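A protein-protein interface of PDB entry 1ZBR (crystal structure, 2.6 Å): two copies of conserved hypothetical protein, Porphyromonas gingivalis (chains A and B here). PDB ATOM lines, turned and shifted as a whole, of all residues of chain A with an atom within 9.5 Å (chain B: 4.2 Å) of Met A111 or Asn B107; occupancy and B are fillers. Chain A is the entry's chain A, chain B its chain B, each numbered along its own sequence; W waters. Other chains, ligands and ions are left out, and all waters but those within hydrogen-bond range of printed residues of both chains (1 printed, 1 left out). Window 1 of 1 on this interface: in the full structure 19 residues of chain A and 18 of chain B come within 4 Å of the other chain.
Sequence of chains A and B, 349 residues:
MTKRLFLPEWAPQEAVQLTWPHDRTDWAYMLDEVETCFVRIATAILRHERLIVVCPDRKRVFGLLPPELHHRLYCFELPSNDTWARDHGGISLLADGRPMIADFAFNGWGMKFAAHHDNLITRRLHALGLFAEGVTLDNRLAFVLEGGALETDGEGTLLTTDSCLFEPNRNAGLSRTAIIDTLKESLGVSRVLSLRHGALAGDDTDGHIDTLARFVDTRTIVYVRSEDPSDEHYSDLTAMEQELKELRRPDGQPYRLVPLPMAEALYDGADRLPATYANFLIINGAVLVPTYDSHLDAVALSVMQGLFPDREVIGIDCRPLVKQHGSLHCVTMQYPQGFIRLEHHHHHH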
ATOM      1  N   ALA A 105      24.552   3.462   8.118  1.00  0.00           N
ATOM      2  CA  ALA A 105      25.097   4.772   7.838  1.00  0.00           C
ATOM      3  C   ALA A 105      24.029   5.618   7.160  1.00  0.00           C
ATOM      4  O   ALA A 105      23.224   5.118   6.372  1.00  0.00           O
ATOM      5  CB  ALA A 105      26.319   4.649   6.935  1.00  0.00           C
ATOM      6  N   PHE A 106      24.030   6.904   7.491  1.00  0.00           N
ATOM      7  CA  PHE A 106      23.108   7.889   6.934  1.00  0.00           C
ATOM      8  C   PHE A 106      24.022   9.038   6.498  1.00  0.00           C
ATOM      9  O   PHE A 106      24.790   9.547   7.314  1.00  0.00           O
ATOM     10  CB  PHE A 106      22.133   8.388   8.012  1.00  0.00           C
ATOM     11  CG  PHE A 106      21.469   9.694   7.665  1.00  0.00           C
ATOM     12  CD1 PHE A 106      20.524   9.761   6.652  1.00  0.00           C
ATOM     13  CD2 PHE A 106      21.833  10.864   8.305  1.00  0.00           C
ATOM     14  CE1 PHE A 106      19.960  10.967   6.282  1.00  0.00           C
ATOM     15  CE2 PHE A 106      21.269  12.072   7.938  1.00  0.00           C
ATOM     16  CZ  PHE A 106      20.333  12.116   6.924  1.00  0.00           C
ATOM     17  N   ASN A 107      23.952   9.460   5.241  1.00  0.00           N
ATOM     18  CA  ASN A 107      24.836  10.531   4.804  1.00  0.00           C
ATOM     19  C   ASN A 107      24.158  11.718   4.137  1.00  0.00           C
ATOM     20  O   ASN A 107      24.701  12.319   3.209  1.00  0.00           O
ATOM     21  CB  ASN A 107      25.917   9.963   3.886  1.00  0.00           C
ATOM     22  CG  ASN A 107      25.344   9.184   2.714  1.00  0.00           C
ATOM     23  OD1 ASN A 107      26.086   8.560   1.958  1.00  0.00           O
ATOM     24  ND2 ASN A 107      24.016   9.222   2.552  1.00  0.00           N
ATOM     25  N   GLY A 108      22.975  12.052   4.634  1.00  0.00           N
ATOM     26  CA  GLY A 108      22.231  13.174   4.109  1.00  0.00           C
ATOM     27  C   GLY A 108      21.522  12.841   2.817  1.00  0.00           C
ATOM     28  O   GLY A 108      21.420  13.681   1.926  1.00  0.00           O
ATOM     29  N   TRP A 109      21.032  11.610   2.712  1.00  0.00           N
ATOM     30  CA  TRP A 109      20.329  11.175   1.515  1.00  0.00           C
ATOM     31  C   TRP A 109      21.217  11.331   0.284  1.00  0.00           C
ATOM     32  O   TRP A 109      20.859  12.023  -0.664  1.00  0.00           O
ATOM     33  CB  TRP A 109      19.063  12.012   1.344  1.00  0.00           C
ATOM     34  CG  TRP A 109      18.212  12.050   2.580  1.00  0.00           C
ATOM     35  CD1 TRP A 109      17.383  11.070   3.032  1.00  0.00           C
ATOM     36  CD2 TRP A 109      18.139  13.114   3.539  1.00  0.00           C
ATOM     37  NE1 TRP A 109      16.803  11.455   4.214  1.00  0.00           N
ATOM     38  CE2 TRP A 109      17.252  12.703   4.549  1.00  0.00           C
ATOM     39  CE3 TRP A 109      18.751  14.372   3.644  1.00  0.00           C
ATOM     40  CZ2 TRP A 109      16.945  13.507   5.648  1.00  0.00           C
ATOM     41  CZ3 TRP A 109      18.446  15.169   4.738  1.00  0.00           C
ATOM     42  CH2 TRP A 109      17.554  14.729   5.728  1.00  0.00           C
ATOM     43  N   GLY A 110      22.376  10.691   0.304  1.00  0.00           N
ATOM     44  CA  GLY A 110      23.273  10.783  -0.827  1.00  0.00           C
ATOM     45  C   GLY A 110      24.205  11.980  -0.780  1.00  0.00           C
ATOM     46  O   GLY A 110      24.602  12.505  -1.827  1.00  0.00           O
ATOM     47  N   MET A 111      24.545  12.413   0.434  1.00  0.00           N
ATOM     48  CA  MET A 111      25.450  13.542   0.653  1.00  0.00           C
ATOM     49  C   MET A 111      24.892  14.885   0.168  1.00  0.00           C
ATOM     50  O   MET A 111      25.650  15.780  -0.221  1.00  0.00           O
ATOM     51  CB  MET A 111      26.793  13.270  -0.021  1.00  0.00           C
ATOM     52  CG  MET A 111      27.489  12.004   0.437  1.00  0.00           C
ATOM     53  SD  MET A 111      28.949  11.525  -0.760  1.00  0.00           S
ATOM     54  CE  MET A 111      28.554   9.643  -1.066  1.00  0.00           C
ATOM     55  N   LYS A 112      23.565  15.010   0.187  1.00  0.00           N
ATOM     56  CA  LYS A 112      22.889  16.244  -0.211  1.00  0.00           C
ATOM     57  C   LYS A 112      22.994  17.288   0.909  1.00  0.00           C
ATOM     58  O   LYS A 112      22.870  18.484   0.668  1.00  0.00           O
ATOM     59  CB  LYS A 112      21.408  15.984  -0.489  1.00  0.00           C
ATOM     60  CG  LYS A 112      21.020  15.826  -1.938  1.00  0.00           C
ATOM     61  CD  LYS A 112      21.305  14.442  -2.443  1.00  0.00           C
ATOM     62  CE  LYS A 112      20.106  13.922  -3.211  1.00  0.00           C
ATOM     63  NZ  LYS A 112      18.906  13.905  -2.334  1.00  0.00           N
ATOM     64  N   PHE A 113      23.190  16.835   2.141  1.00  0.00           N
ATOM     65  CA  PHE A 113      23.317  17.760   3.254  1.00  0.00           C
ATOM     66  C   PHE A 113      24.275  17.182   4.294  1.00  0.00           C
ATOM     67  O   PHE A 113      24.503  15.962   4.336  1.00  0.00           O
ATOM     68  CB  PHE A 113      21.961  18.030   3.919  1.00  0.00           C
ATOM     69  CG  PHE A 113      20.840  18.394   2.959  1.00  0.00           C
ATOM     70  CD1 PHE A 113      20.132  17.405   2.282  1.00  0.00           C
ATOM     71  CD2 PHE A 113      20.432  19.716   2.808  1.00  0.00           C
ATOM     72  CE1 PHE A 113      19.030  17.729   1.485  1.00  0.00           C
ATOM     73  CE2 PHE A 113      19.335  20.043   2.012  1.00  0.00           C
ATOM     74  CZ  PHE A 113      18.634  19.050   1.355  1.00  0.00           C
ATOM     75  N   ALA A 114      24.834  18.057   5.131  1.00  0.00           N
ATOM     76  CA  ALA A 114      25.764  17.626   6.177  1.00  0.00           C
ATOM     77  C   ALA A 114      25.073  16.652   7.136  1.00  0.00           C
ATOM     78  O   ALA A 114      23.914  16.837   7.503  1.00  0.00           O
ATOM     79  CB  ALA A 114      26.294  18.828   6.942  1.00  0.00           C
ATOM     80  N   ALA A 115      25.799  15.623   7.554  1.00  0.00           N
ATOM     81  CA  ALA A 115      25.226  14.615   8.423  1.00  0.00           C
ATOM     82  C   ALA A 115      26.204  14.055   9.432  1.00  0.00           C
ATOM     83  O   ALA A 115      25.978  12.992  10.022  1.00  0.00           O
ATOM     84  CB  ALA A 115      24.670  13.491   7.578  1.00  0.00           C
ATOM     85  N   HIS A 116      27.299  14.767   9.640  1.00  0.00           N
ATOM     86  CA  HIS A 116      28.316  14.313  10.578  1.00  0.00           C
ATOM     87  C   HIS A 116      27.788  14.170  12.020  1.00  0.00           C
ATOM     88  O   HIS A 116      28.343  13.412  12.812  1.00  0.00           O
ATOM     89  CB  HIS A 116      29.531  15.254  10.507  1.00  0.00           C
ATOM     90  CG  HIS A 116      29.244  16.650  10.950  1.00  0.00           C
ATOM     91  ND1 HIS A 116      28.091  17.321  10.598  1.00  0.00           N
ATOM     92  CD2 HIS A 116      29.948  17.497  11.736  1.00  0.00           C
ATOM     93  CE1 HIS A 116      28.097  18.519  11.153  1.00  0.00           C
ATOM     94  NE2 HIS A 116      29.214  18.650  11.850  1.00  0.00           N
ATOM     95  N   ASN A 119      24.559  11.046  11.895  1.00  0.00           N
ATOM     96  CA  ASN A 119      25.068   9.695  11.720  1.00  0.00           C
ATOM     97  C   ASN A 119      25.817   9.234  12.965  1.00  0.00           C
ATOM     98  O   ASN A 119      26.530   8.231  12.943  1.00  0.00           O
ATOM     99  CB  ASN A 119      25.994   9.649  10.504  1.00  0.00           C
ATOM    100  CG  ASN A 119      26.431   8.251  10.166  1.00  0.00           C
ATOM    101  OD1 ASN A 119      27.599   7.907  10.293  1.00  0.00           O
ATOM    102  ND2 ASN A 119      25.489   7.428   9.738  1.00  0.00           N
ATOM    103  N   LEU A 141      27.737   0.557   9.691  1.00  0.00           N
ATOM    104  CA  LEU A 141      28.148   1.854   9.153  1.00  0.00           C
ATOM    105  C   LEU A 141      28.831   1.743   7.790  1.00  0.00           C
ATOM    106  O   LEU A 141      29.002   2.737   7.096  1.00  0.00           O
ATOM    107  CB  LEU A 141      29.062   2.576  10.150  1.00  0.00           C
ATOM    108  CG  LEU A 141      28.512   2.972  11.527  1.00  0.00           C
ATOM    109  CD1 LEU A 141      29.672   3.487  12.357  1.00  0.00           C
ATOM    110  CD2 LEU A 141      27.416   4.039  11.420  1.00  0.00           C
ATOM    111  N   VAL A 144      25.359   2.366   3.549  1.00  0.00           N
ATOM    112  CA  VAL A 144      24.476   3.528   3.663  1.00  0.00           C
ATOM    113  C   VAL A 144      23.006   3.102   3.544  1.00  0.00           C
ATOM    114  O   VAL A 144      22.608   2.478   2.556  1.00  0.00           O
ATOM    115  CB  VAL A 144      24.771   4.584   2.567  1.00  0.00           C
ATOM    116  CG1 VAL A 144      23.812   5.773   2.701  1.00  0.00           C
ATOM    117  CG2 VAL A 144      26.200   5.052   2.672  1.00  0.00           C
ATOM    118  N   GLU A 146      18.776   4.279   5.044  1.00  0.00           N
ATOM    119  CA  GLU A 146      17.880   5.005   5.923  1.00  0.00           C
ATOM    120  C   GLU A 146      16.537   4.295   6.050  1.00  0.00           C
ATOM    121  O   GLU A 146      15.980   3.812   5.069  1.00  0.00           O
ATOM    122  CB  GLU A 146      17.691   6.447   5.426  1.00  0.00           C
ATOM    123  CG  GLU A 146      17.356   6.582   3.949  1.00  0.00           C
ATOM    124  CD  GLU A 146      18.575   6.557   3.047  1.00  0.00           C
ATOM    125  OE1 GLU A 146      19.148   7.640   2.814  1.00  0.00           O
ATOM    126  OE2 GLU A 146      18.958   5.457   2.582  1.00  0.00           O
ATOM    127  N   GLU A 167      20.947   4.762  -5.776  1.00  0.00           N
ATOM    128  CA  GLU A 167      21.378   6.160  -5.864  1.00  0.00           C
ATOM    129  C   GLU A 167      22.906   6.137  -5.953  1.00  0.00           C
ATOM    130  O   GLU A 167      23.560   5.400  -5.227  1.00  0.00           O
ATOM    131  CB  GLU A 167      20.932   6.912  -4.604  1.00  0.00           C
ATOM    132  CG  GLU A 167      21.931   7.951  -4.055  1.00  0.00           C
ATOM    133  CD  GLU A 167      21.870   9.258  -4.795  1.00  0.00           C
ATOM    134  OE1 GLU A 167      20.775   9.579  -5.304  1.00  0.00           O
ATOM    135  OE2 GLU A 167      22.897   9.968  -4.857  1.00  0.00           O
ATOM    136  N   PRO A 168      23.494   6.945  -6.840  1.00  0.00           N
ATOM    137  CA  PRO A 168      24.954   6.978  -6.994  1.00  0.00           C
ATOM    138  C   PRO A 168      25.797   7.373  -5.773  1.00  0.00           C
ATOM    139  O   PRO A 168      26.999   7.133  -5.759  1.00  0.00           O
ATOM    140  CB  PRO A 168      25.153   7.918  -8.189  1.00  0.00           C
ATOM    141  CG  PRO A 168      23.942   8.783  -8.151  1.00  0.00           C
ATOM    142  CD  PRO A 168      22.846   7.804  -7.842  1.00  0.00           C
ATOM    143  N   ASN A 169      25.176   7.961  -4.754  1.00  0.00           N
ATOM    144  CA  ASN A 169      25.918   8.353  -3.564  1.00  0.00           C
ATOM    145  C   ASN A 169      25.500   7.545  -2.352  1.00  0.00           C
ATOM    146  O   ASN A 169      25.835   7.888  -1.229  1.00  0.00           O
ATOM    147  CB  ASN A 169      25.754   9.849  -3.282  1.00  0.00           C
ATOM    148  CG  ASN A 169      26.492  10.721  -4.304  1.00  0.00           C
ATOM    149  OD1 ASN A 169      27.661  10.466  -4.620  1.00  0.00           O
ATOM    150  ND2 ASN A 169      25.818  11.750  -4.821  1.00  0.00           N
ATOM    151  N   ARG A 170      24.760   6.469  -2.584  1.00  0.00           N
ATOM    152  CA  ARG A 170      24.335   5.607  -1.497  1.00  0.00           C
ATOM    153  C   ARG A 170      25.415   4.549  -1.344  1.00  0.00           C
ATOM    154  O   ARG A 170      26.343   4.713  -0.554  1.00  0.00           O
ATOM    155  CB  ARG A 170      22.996   4.953  -1.831  1.00  0.00           C
ATOM    156  CG  ARG A 170      21.819   5.437  -0.984  1.00  0.00           C
ATOM    157  CD  ARG A 170      21.629   6.943  -1.046  1.00  0.00           C
ATOM    158  NE  ARG A 170      20.391   7.351  -0.382  1.00  0.00           N
ATOM    159  CZ  ARG A 170      19.598   8.329  -0.817  1.00  0.00           C
ATOM    160  NH1 ARG A 170      18.495   8.628  -0.158  1.00  0.00           N
ATOM    161  NH2 ARG A 170      19.909   9.006  -1.916  1.00  0.00           N
ATOM    162  N   ASN A 171      25.297   3.475  -2.119  1.00  0.00           N
ATOM    163  CA  ASN A 171      26.267   2.383  -2.093  1.00  0.00           C
ATOM    164  C   ASN A 171      26.765   2.033  -3.511  1.00  0.00           C
ATOM    165  O   ASN A 171      26.719   0.873  -3.934  1.00  0.00           O
ATOM    166  CB  ASN A 171      25.635   1.150  -1.450  1.00  0.00           C
ATOM    167  CG  ASN A 171      25.346   1.338   0.027  1.00  0.00           C
ATOM    168  OD1 ASN A 171      26.251   1.564   0.836  1.00  0.00           O
ATOM    169  ND2 ASN A 171      24.078   1.233   0.390  1.00  0.00           N
ATOM    170  N   ALA A 172      27.238   3.038  -4.244  1.00  0.00           N
ATOM    171  CA  ALA A 172      27.740   2.819  -5.600  1.00  0.00           C
ATOM    172  C   ALA A 172      28.985   1.927  -5.580  1.00  0.00           C
ATOM    173  O   ALA A 172      29.340   1.313  -6.586  1.00  0.00           O
ATOM    174  CB  ALA A 172      28.053   4.162  -6.274  1.00  0.00           C
ATOM    175  N   GLY A 173      29.651   1.865  -4.432  1.00  0.00           N
ATOM    176  CA  GLY A 173      30.828   1.018  -4.313  1.00  0.00           C
ATOM    177  C   GLY A 173      30.455  -0.447  -4.442  1.00  0.00           C
ATOM    178  O   GLY A 173      31.321  -1.316  -4.591  1.00  0.00           O
ATOM    179  N   ASP A 204      13.176  14.825  -1.948  1.00  0.00           N
ATOM    180  CA  ASP A 204      14.635  14.908  -1.985  1.00  0.00           C
ATOM    181  C   ASP A 204      15.303  13.644  -1.468  1.00  0.00           C
ATOM    182  O   ASP A 204      16.524  13.572  -1.412  1.00  0.00           O
ATOM    183  CB  ASP A 204      15.144  16.090  -1.162  1.00  0.00           C
ATOM    184  CG  ASP A 204      15.172  17.376  -1.945  1.00  0.00           C
ATOM    185  OD1 ASP A 204      15.176  17.313  -3.205  1.00  0.00           O
ATOM    186  OD2 ASP A 204      15.212  18.455  -1.299  1.00  0.00           O
ATOM    187  N   ASP A 206      15.008  10.849  -2.918  1.00  0.00           N
ATOM    188  CA  ASP A 206      15.181   9.995  -4.089  1.00  0.00           C
ATOM    189  C   ASP A 206      14.124   8.904  -4.171  1.00  0.00           C
ATOM    190  O   ASP A 206      14.420   7.765  -4.531  1.00  0.00           O
ATOM    191  CB  ASP A 206      16.573   9.367  -4.085  1.00  0.00           C
ATOM    192  CG  ASP A 206      17.660  10.390  -4.270  1.00  0.00           C
ATOM    193  OD1 ASP A 206      17.721  10.998  -5.360  1.00  0.00           O
ATOM    194  OD2 ASP A 206      18.453  10.596  -3.327  1.00  0.00           O
ATOM    195  N   ALA B 105      35.819   7.219  -2.365  1.00  0.00           N
ATOM    196  CA  ALA B 105      34.664   8.006  -1.966  1.00  0.00           C
ATOM    197  C   ALA B 105      35.007   9.243  -1.125  1.00  0.00           C
ATOM    198  O   ALA B 105      35.802   9.195  -0.182  1.00  0.00           O
ATOM    199  CB  ALA B 105      33.674   7.115  -1.194  1.00  0.00           C
ATOM    200  N   PHE B 106      34.370  10.349  -1.471  1.00  0.00           N
ATOM    201  CA  PHE B 106      34.552  11.597  -0.755  1.00  0.00           C
ATOM    202  C   PHE B 106      33.178  11.999  -0.227  1.00  0.00           C
ATOM    203  O   PHE B 106      32.259  12.194  -1.017  1.00  0.00           O
ATOM    204  CB  PHE B 106      35.054  12.674  -1.696  1.00  0.00           C
ATOM    205  CG  PHE B 106      35.061  14.025  -1.084  1.00  0.00           C
ATOM    206  CD1 PHE B 106      36.021  14.364  -0.140  1.00  0.00           C
ATOM    207  CD2 PHE B 106      34.079  14.946  -1.410  1.00  0.00           C
ATOM    208  CE1 PHE B 106      36.005  15.612   0.480  1.00  0.00           C
ATOM    209  CE2 PHE B 106      34.047  16.195  -0.800  1.00  0.00           C
ATOM    210  CZ  PHE B 106      35.016  16.528   0.150  1.00  0.00           C
ATOM    211  N   ASN B 107      33.036  12.114   1.095  1.00  0.00           N
ATOM    212  CA  ASN B 107      31.763  12.490   1.701  1.00  0.00           C
ATOM    213  C   ASN B 107      31.794  13.760   2.546  1.00  0.00           C
ATOM    214  O   ASN B 107      31.234  13.799   3.639  1.00  0.00           O
ATOM    215  CB  ASN B 107      31.182  11.326   2.532  1.00  0.00           C
ATOM    216  CG  ASN B 107      32.085  10.876   3.702  1.00  0.00           C
ATOM    217  OD1 ASN B 107      31.796   9.865   4.346  1.00  0.00           O
ATOM    218  ND2 ASN B 107      33.150  11.615   3.980  1.00  0.00           N
ATOM    219  N   GLY B 108      32.449  14.801   2.042  1.00  0.00           N
ATOM    220  CA  GLY B 108      32.498  16.067   2.762  1.00  0.00           C
ATOM    221  C   GLY B 108      33.346  16.093   4.020  1.00  0.00           C
ATOM    222  O   GLY B 108      33.065  16.844   4.951  1.00  0.00           O
ATOM    223  N   TRP B 109      34.390  15.271   4.044  1.00  0.00           N
ATOM    224  CA  TRP B 109      35.304  15.208   5.179  1.00  0.00           C
ATOM    225  C   TRP B 109      34.589  14.718   6.427  1.00  0.00           C
ATOM    226  O   TRP B 109      34.628  15.359   7.479  1.00  0.00           O
ATOM    227  CB  TRP B 109      35.912  16.589   5.431  1.00  0.00           C
ATOM    228  CG  TRP B 109      36.612  17.157   4.232  1.00  0.00           C
ATOM    229  CD1 TRP B 109      37.897  16.914   3.831  1.00  0.00           C
ATOM    230  CD2 TRP B 109      36.061  18.068   3.271  1.00  0.00           C
ATOM    231  NE1 TRP B 109      38.180  17.625   2.690  1.00  0.00           N
ATOM    232  CE2 TRP B 109      37.071  18.345   2.331  1.00  0.00           C
ATOM    233  CE3 TRP B 109      34.816  18.687   3.125  1.00  0.00           C
ATOM    234  CZ2 TRP B 109      36.865  19.202   1.245  1.00  0.00           C
ATOM    235  CZ3 TRP B 109      34.613  19.539   2.044  1.00  0.00           C
ATOM    236  CH2 TRP B 109      35.635  19.793   1.126  1.00  0.00           C
ATOM    237  N   GLY B 110      33.945  13.568   6.303  1.00  0.00           N
ATOM    238  CA  GLY B 110      33.233  13.008   7.426  1.00  0.00           C
ATOM    239  C   GLY B 110      31.812  13.524   7.505  1.00  0.00           C
ATOM    240  O   GLY B 110      31.228  13.539   8.586  1.00  0.00           O
ATOM    241  N   MET B 111      31.267  13.961   6.370  1.00  0.00           N
ATOM    242  CA  MET B 111      29.900  14.460   6.294  1.00  0.00           C
ATOM    243  C   MET B 111      29.681  15.858   6.849  1.00  0.00           C
ATOM    244  O   MET B 111      28.560  16.213   7.203  1.00  0.00           O
ATOM    245  CB  MET B 111      28.952  13.486   6.989  1.00  0.00           C
ATOM    246  CG  MET B 111      28.788  12.163   6.270  1.00  0.00           C
ATOM    247  SD  MET B 111      27.802  10.823   7.297  1.00  0.00           S
ATOM    248  CE  MET B 111      28.726   9.201   6.700  1.00  0.00           C
ATOM    249  N   ALA B 114      27.845  19.013   2.441  1.00  0.00           N
ATOM    250  CA  ALA B 114      27.253  18.299   1.321  1.00  0.00           C
ATOM    251  C   ALA B 114      28.337  18.058   0.269  1.00  0.00           C
ATOM    252  O   ALA B 114      29.195  18.916   0.052  1.00  0.00           O
ATOM    253  CB  ALA B 114      26.130  19.135   0.739  1.00  0.00           C
ATOM    254  N   ALA B 115      28.300  16.894  -0.365  1.00  0.00           N
ATOM    255  CA  ALA B 115      29.271  16.540  -1.398  1.00  0.00           C
ATOM    256  C   ALA B 115      28.648  15.646  -2.494  1.00  0.00           C
ATOM    257  O   ALA B 115      29.362  14.966  -3.240  1.00  0.00           O
ATOM    258  CB  ALA B 115      30.450  15.828  -0.763  1.00  0.00           C
ATOM    259  N   HIS B 116      27.322  15.656  -2.593  1.00  0.00           N
ATOM    260  CA  HIS B 116      26.620  14.839  -3.575  1.00  0.00           C
ATOM    261  C   HIS B 116      27.103  15.083  -5.015  1.00  0.00           C
ATOM    262  O   HIS B 116      26.880  14.243  -5.884  1.00  0.00           O
ATOM    263  CB  HIS B 116      25.095  15.047  -3.460  1.00  0.00           C
ATOM    264  CG  HIS B 116      24.642  16.438  -3.780  1.00  0.00           C
ATOM    265  ND1 HIS B 116      25.120  17.551  -3.119  1.00  0.00           N
ATOM    266  CD2 HIS B 116      23.772  16.899  -4.709  1.00  0.00           C
ATOM    267  CE1 HIS B 116      24.568  18.634  -3.630  1.00  0.00           C
ATOM    268  NE2 HIS B 116      23.744  18.268  -4.598  1.00  0.00           N
ATOM    269  N   ASN B 119      31.593  13.833  -5.248  1.00  0.00           N
ATOM    270  CA  ASN B 119      31.827  12.384  -5.281  1.00  0.00           C
ATOM    271  C   ASN B 119      31.349  11.748  -6.593  1.00  0.00           C
ATOM    272  O   ASN B 119      31.259  10.522  -6.721  1.00  0.00           O
ATOM    273  CB  ASN B 119      31.088  11.717  -4.122  1.00  0.00           C
ATOM    274  CG  ASN B 119      31.536  10.290  -3.893  1.00  0.00           C
ATOM    275  OD1 ASN B 119      30.727   9.416  -3.552  1.00  0.00           O
ATOM    276  ND2 ASN B 119      32.837  10.045  -4.068  1.00  0.00           N
ATOM    277  N   VAL B 144      35.672   5.429   2.027  1.00  0.00           N
ATOM    278  CA  VAL B 144      35.909   6.867   2.076  1.00  0.00           C
ATOM    279  C   VAL B 144      37.404   7.141   2.262  1.00  0.00           C
ATOM    280  O   VAL B 144      38.036   6.579   3.157  1.00  0.00           O
ATOM    281  CB  VAL B 144      35.153   7.497   3.238  1.00  0.00           C
ATOM    282  CG1 VAL B 144      35.512   8.960   3.364  1.00  0.00           C
ATOM    283  CG2 VAL B 144      33.678   7.298   3.037  1.00  0.00           C
ATOM    284  N   ASN B 169      33.086   9.062  10.998  1.00  0.00           N
ATOM    285  CA  ASN B 169      32.172   9.208   9.877  1.00  0.00           C
ATOM    286  C   ASN B 169      32.832   8.973   8.546  1.00  0.00           C
ATOM    287  O   ASN B 169      32.402   9.518   7.528  1.00  0.00           O
ATOM    288  CB  ASN B 169      31.514  10.577   9.890  1.00  0.00           C
ATOM    289  CG  ASN B 169      30.438  10.675  10.949  1.00  0.00           C
ATOM    290  OD1 ASN B 169      29.554   9.810  11.026  1.00  0.00           O
ATOM    291  ND2 ASN B 169      30.499  11.721  11.772  1.00  0.00           N
HETATM  292  O   HOH W   1      28.850   8.459   3.104  1.00  0.00           O
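The side-chain carboxylate (OD2) of Asp A206 lies within salt-bridge range of the side-chain amino group (NZ) of Lys A112, 3.5 Å away. O of Asn B169 lies close to OD1 of Asn B107, 3.3 Å away. The backbone NH (N) of Phe A106 sits close to the side-chain amide nitrogen (ND2) of Asn A119. O of Gly A110 lies close to ND2 of Asn A169 (3.3 Å). The backbone carbonyl oxygen (O) of Asp A204 sits at hydrogen-bond distance from the side-chain amino group (NZ) of Lys A112, 2.6 Å away.
Among the printed residues, pairs that only touch across the chains: Gly A110 with His B116 (3.1 Å), His A116 with Gly B110 (3.1 Å), Ala A114 with Met B111 (3.3 Å), Met A111 with Asn B119 (3.3 Å), Lys A112 with Ala B114 (3.3 Å), Met A111 with Ala B114 (3.4 Å), Met A111 with Asn B107 (3.9 Å), Asn A119 with Met B111 (3.9 Å), Asn A107 with Met B111 (3.9 Å), Lys A112 with His B116 (3.9 Å) and Phe A113 with Ala B114 (3.99 Å).
Phe A106 touches Met B111, and with the chains exchanged Met A111 touches Phe B106. Gly A110 touches His B116, and with the chains exchanged His A116 touches Gly B110. His A116 touches Asn B169, and with the chains exchanged Asn A169 touches His B116. Positions printed for both chains: 105, 106, 107, 108, 109, 110, 111, 114, 115, 116, 119, 144 and 169.
Of the 13 printed residues of chain B, 9 touch a printed residue of chain A. Printed residues of chain A that touch a printed residue of chain B: Phe A106, Asn A107, Gly A110, Met A111, Lys A112, Phe A113, Ala A114, Ala A115, His A116, Asn A119 and Asn A169. Among the printed residues, no Asp or Glu carboxylate lies within 4 Å of a Lys or Arg side-chain nitrogen of the other chain.
Of chain B, only Phe B106, Asn B107, Ala B114, Ala B115, His B116 and Asn B119 come within 4 Å of Met A111. Printed residues of chain A within 4 Å of Asn B107: Met A111 (3.9 Å). Of chain A, only Met A111 (3.4 Å) comes within 4 Å of Phe B106. No residue of chain A comes within 4 Å of Gly B108. Met B111 touches just these residues of chain A: Phe A106 (3.3 Å), Asn A107 (3.9 Å), Ala A114 (3.3 Å), Ala A115 (2.8 Å), His A116 (3.1 Å) and Asn A119 (3.9 Å). Of chain A, only Met A111 comes within 4 Å of Ala B115. Printed residues of chain B within 4 Å of Phe A113: Ala B114. Of the printed residues of chain A, Asn B169 touches His A116 (2.9 Å) and Asn A119 (2.8 Å). Printed residues of chain B within 4 Å of Phe A106: Met B111 (3.3 Å). Ala B105 touches none of the printed residues of chain A.
The backbone carbonyl oxygen (O) of Met B111 is in hydrogen-bond range of the backbone NH (N) of Ala A115 (2.8 Å). The backbone NH of His A116 sits at hydrogen-bond distance from the backbone carbonyl oxygen of Met B111, at 3.1 Å. The backbone carbonyl oxygen (O) of Phe B106 lies close to the side-chain sulfur (SD) of Met A111. The side-chain amide oxygen of Asn A169 lies close to the side-chain amide oxygen of Asn B119, 3.4 Å away. The side-chain amide oxygen of Asn A119 sits close to the side-chain amide oxygen of Asn B169 (2.8 Å). The backbone carbonyl oxygen (O) of His A116 is in hydrogen-bond range of the side-chain amide nitrogen (ND2) of Asn B169, at 2.9 Å. The backbone NH (N) of His B116 sits at hydrogen-bond distance from the backbone carbonyl oxygen (O) of Met A111 (2.9 Å). The backbone carbonyl oxygen (O) of Met A111 lies within hydrogen-bond range of the backbone NH (N) of Ala B115, 2.9 Å away. O of His B116 sits at hydrogen-bond distance from ND2 of Asn A169 (2.9 Å). O of Phe A106 sits close to SD of Met B111, at 3.3 Å.
Water W1 bridges OD1 of Asn A107 (3.0 Å) and OD1 of Asn B107 (3.5 Å).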
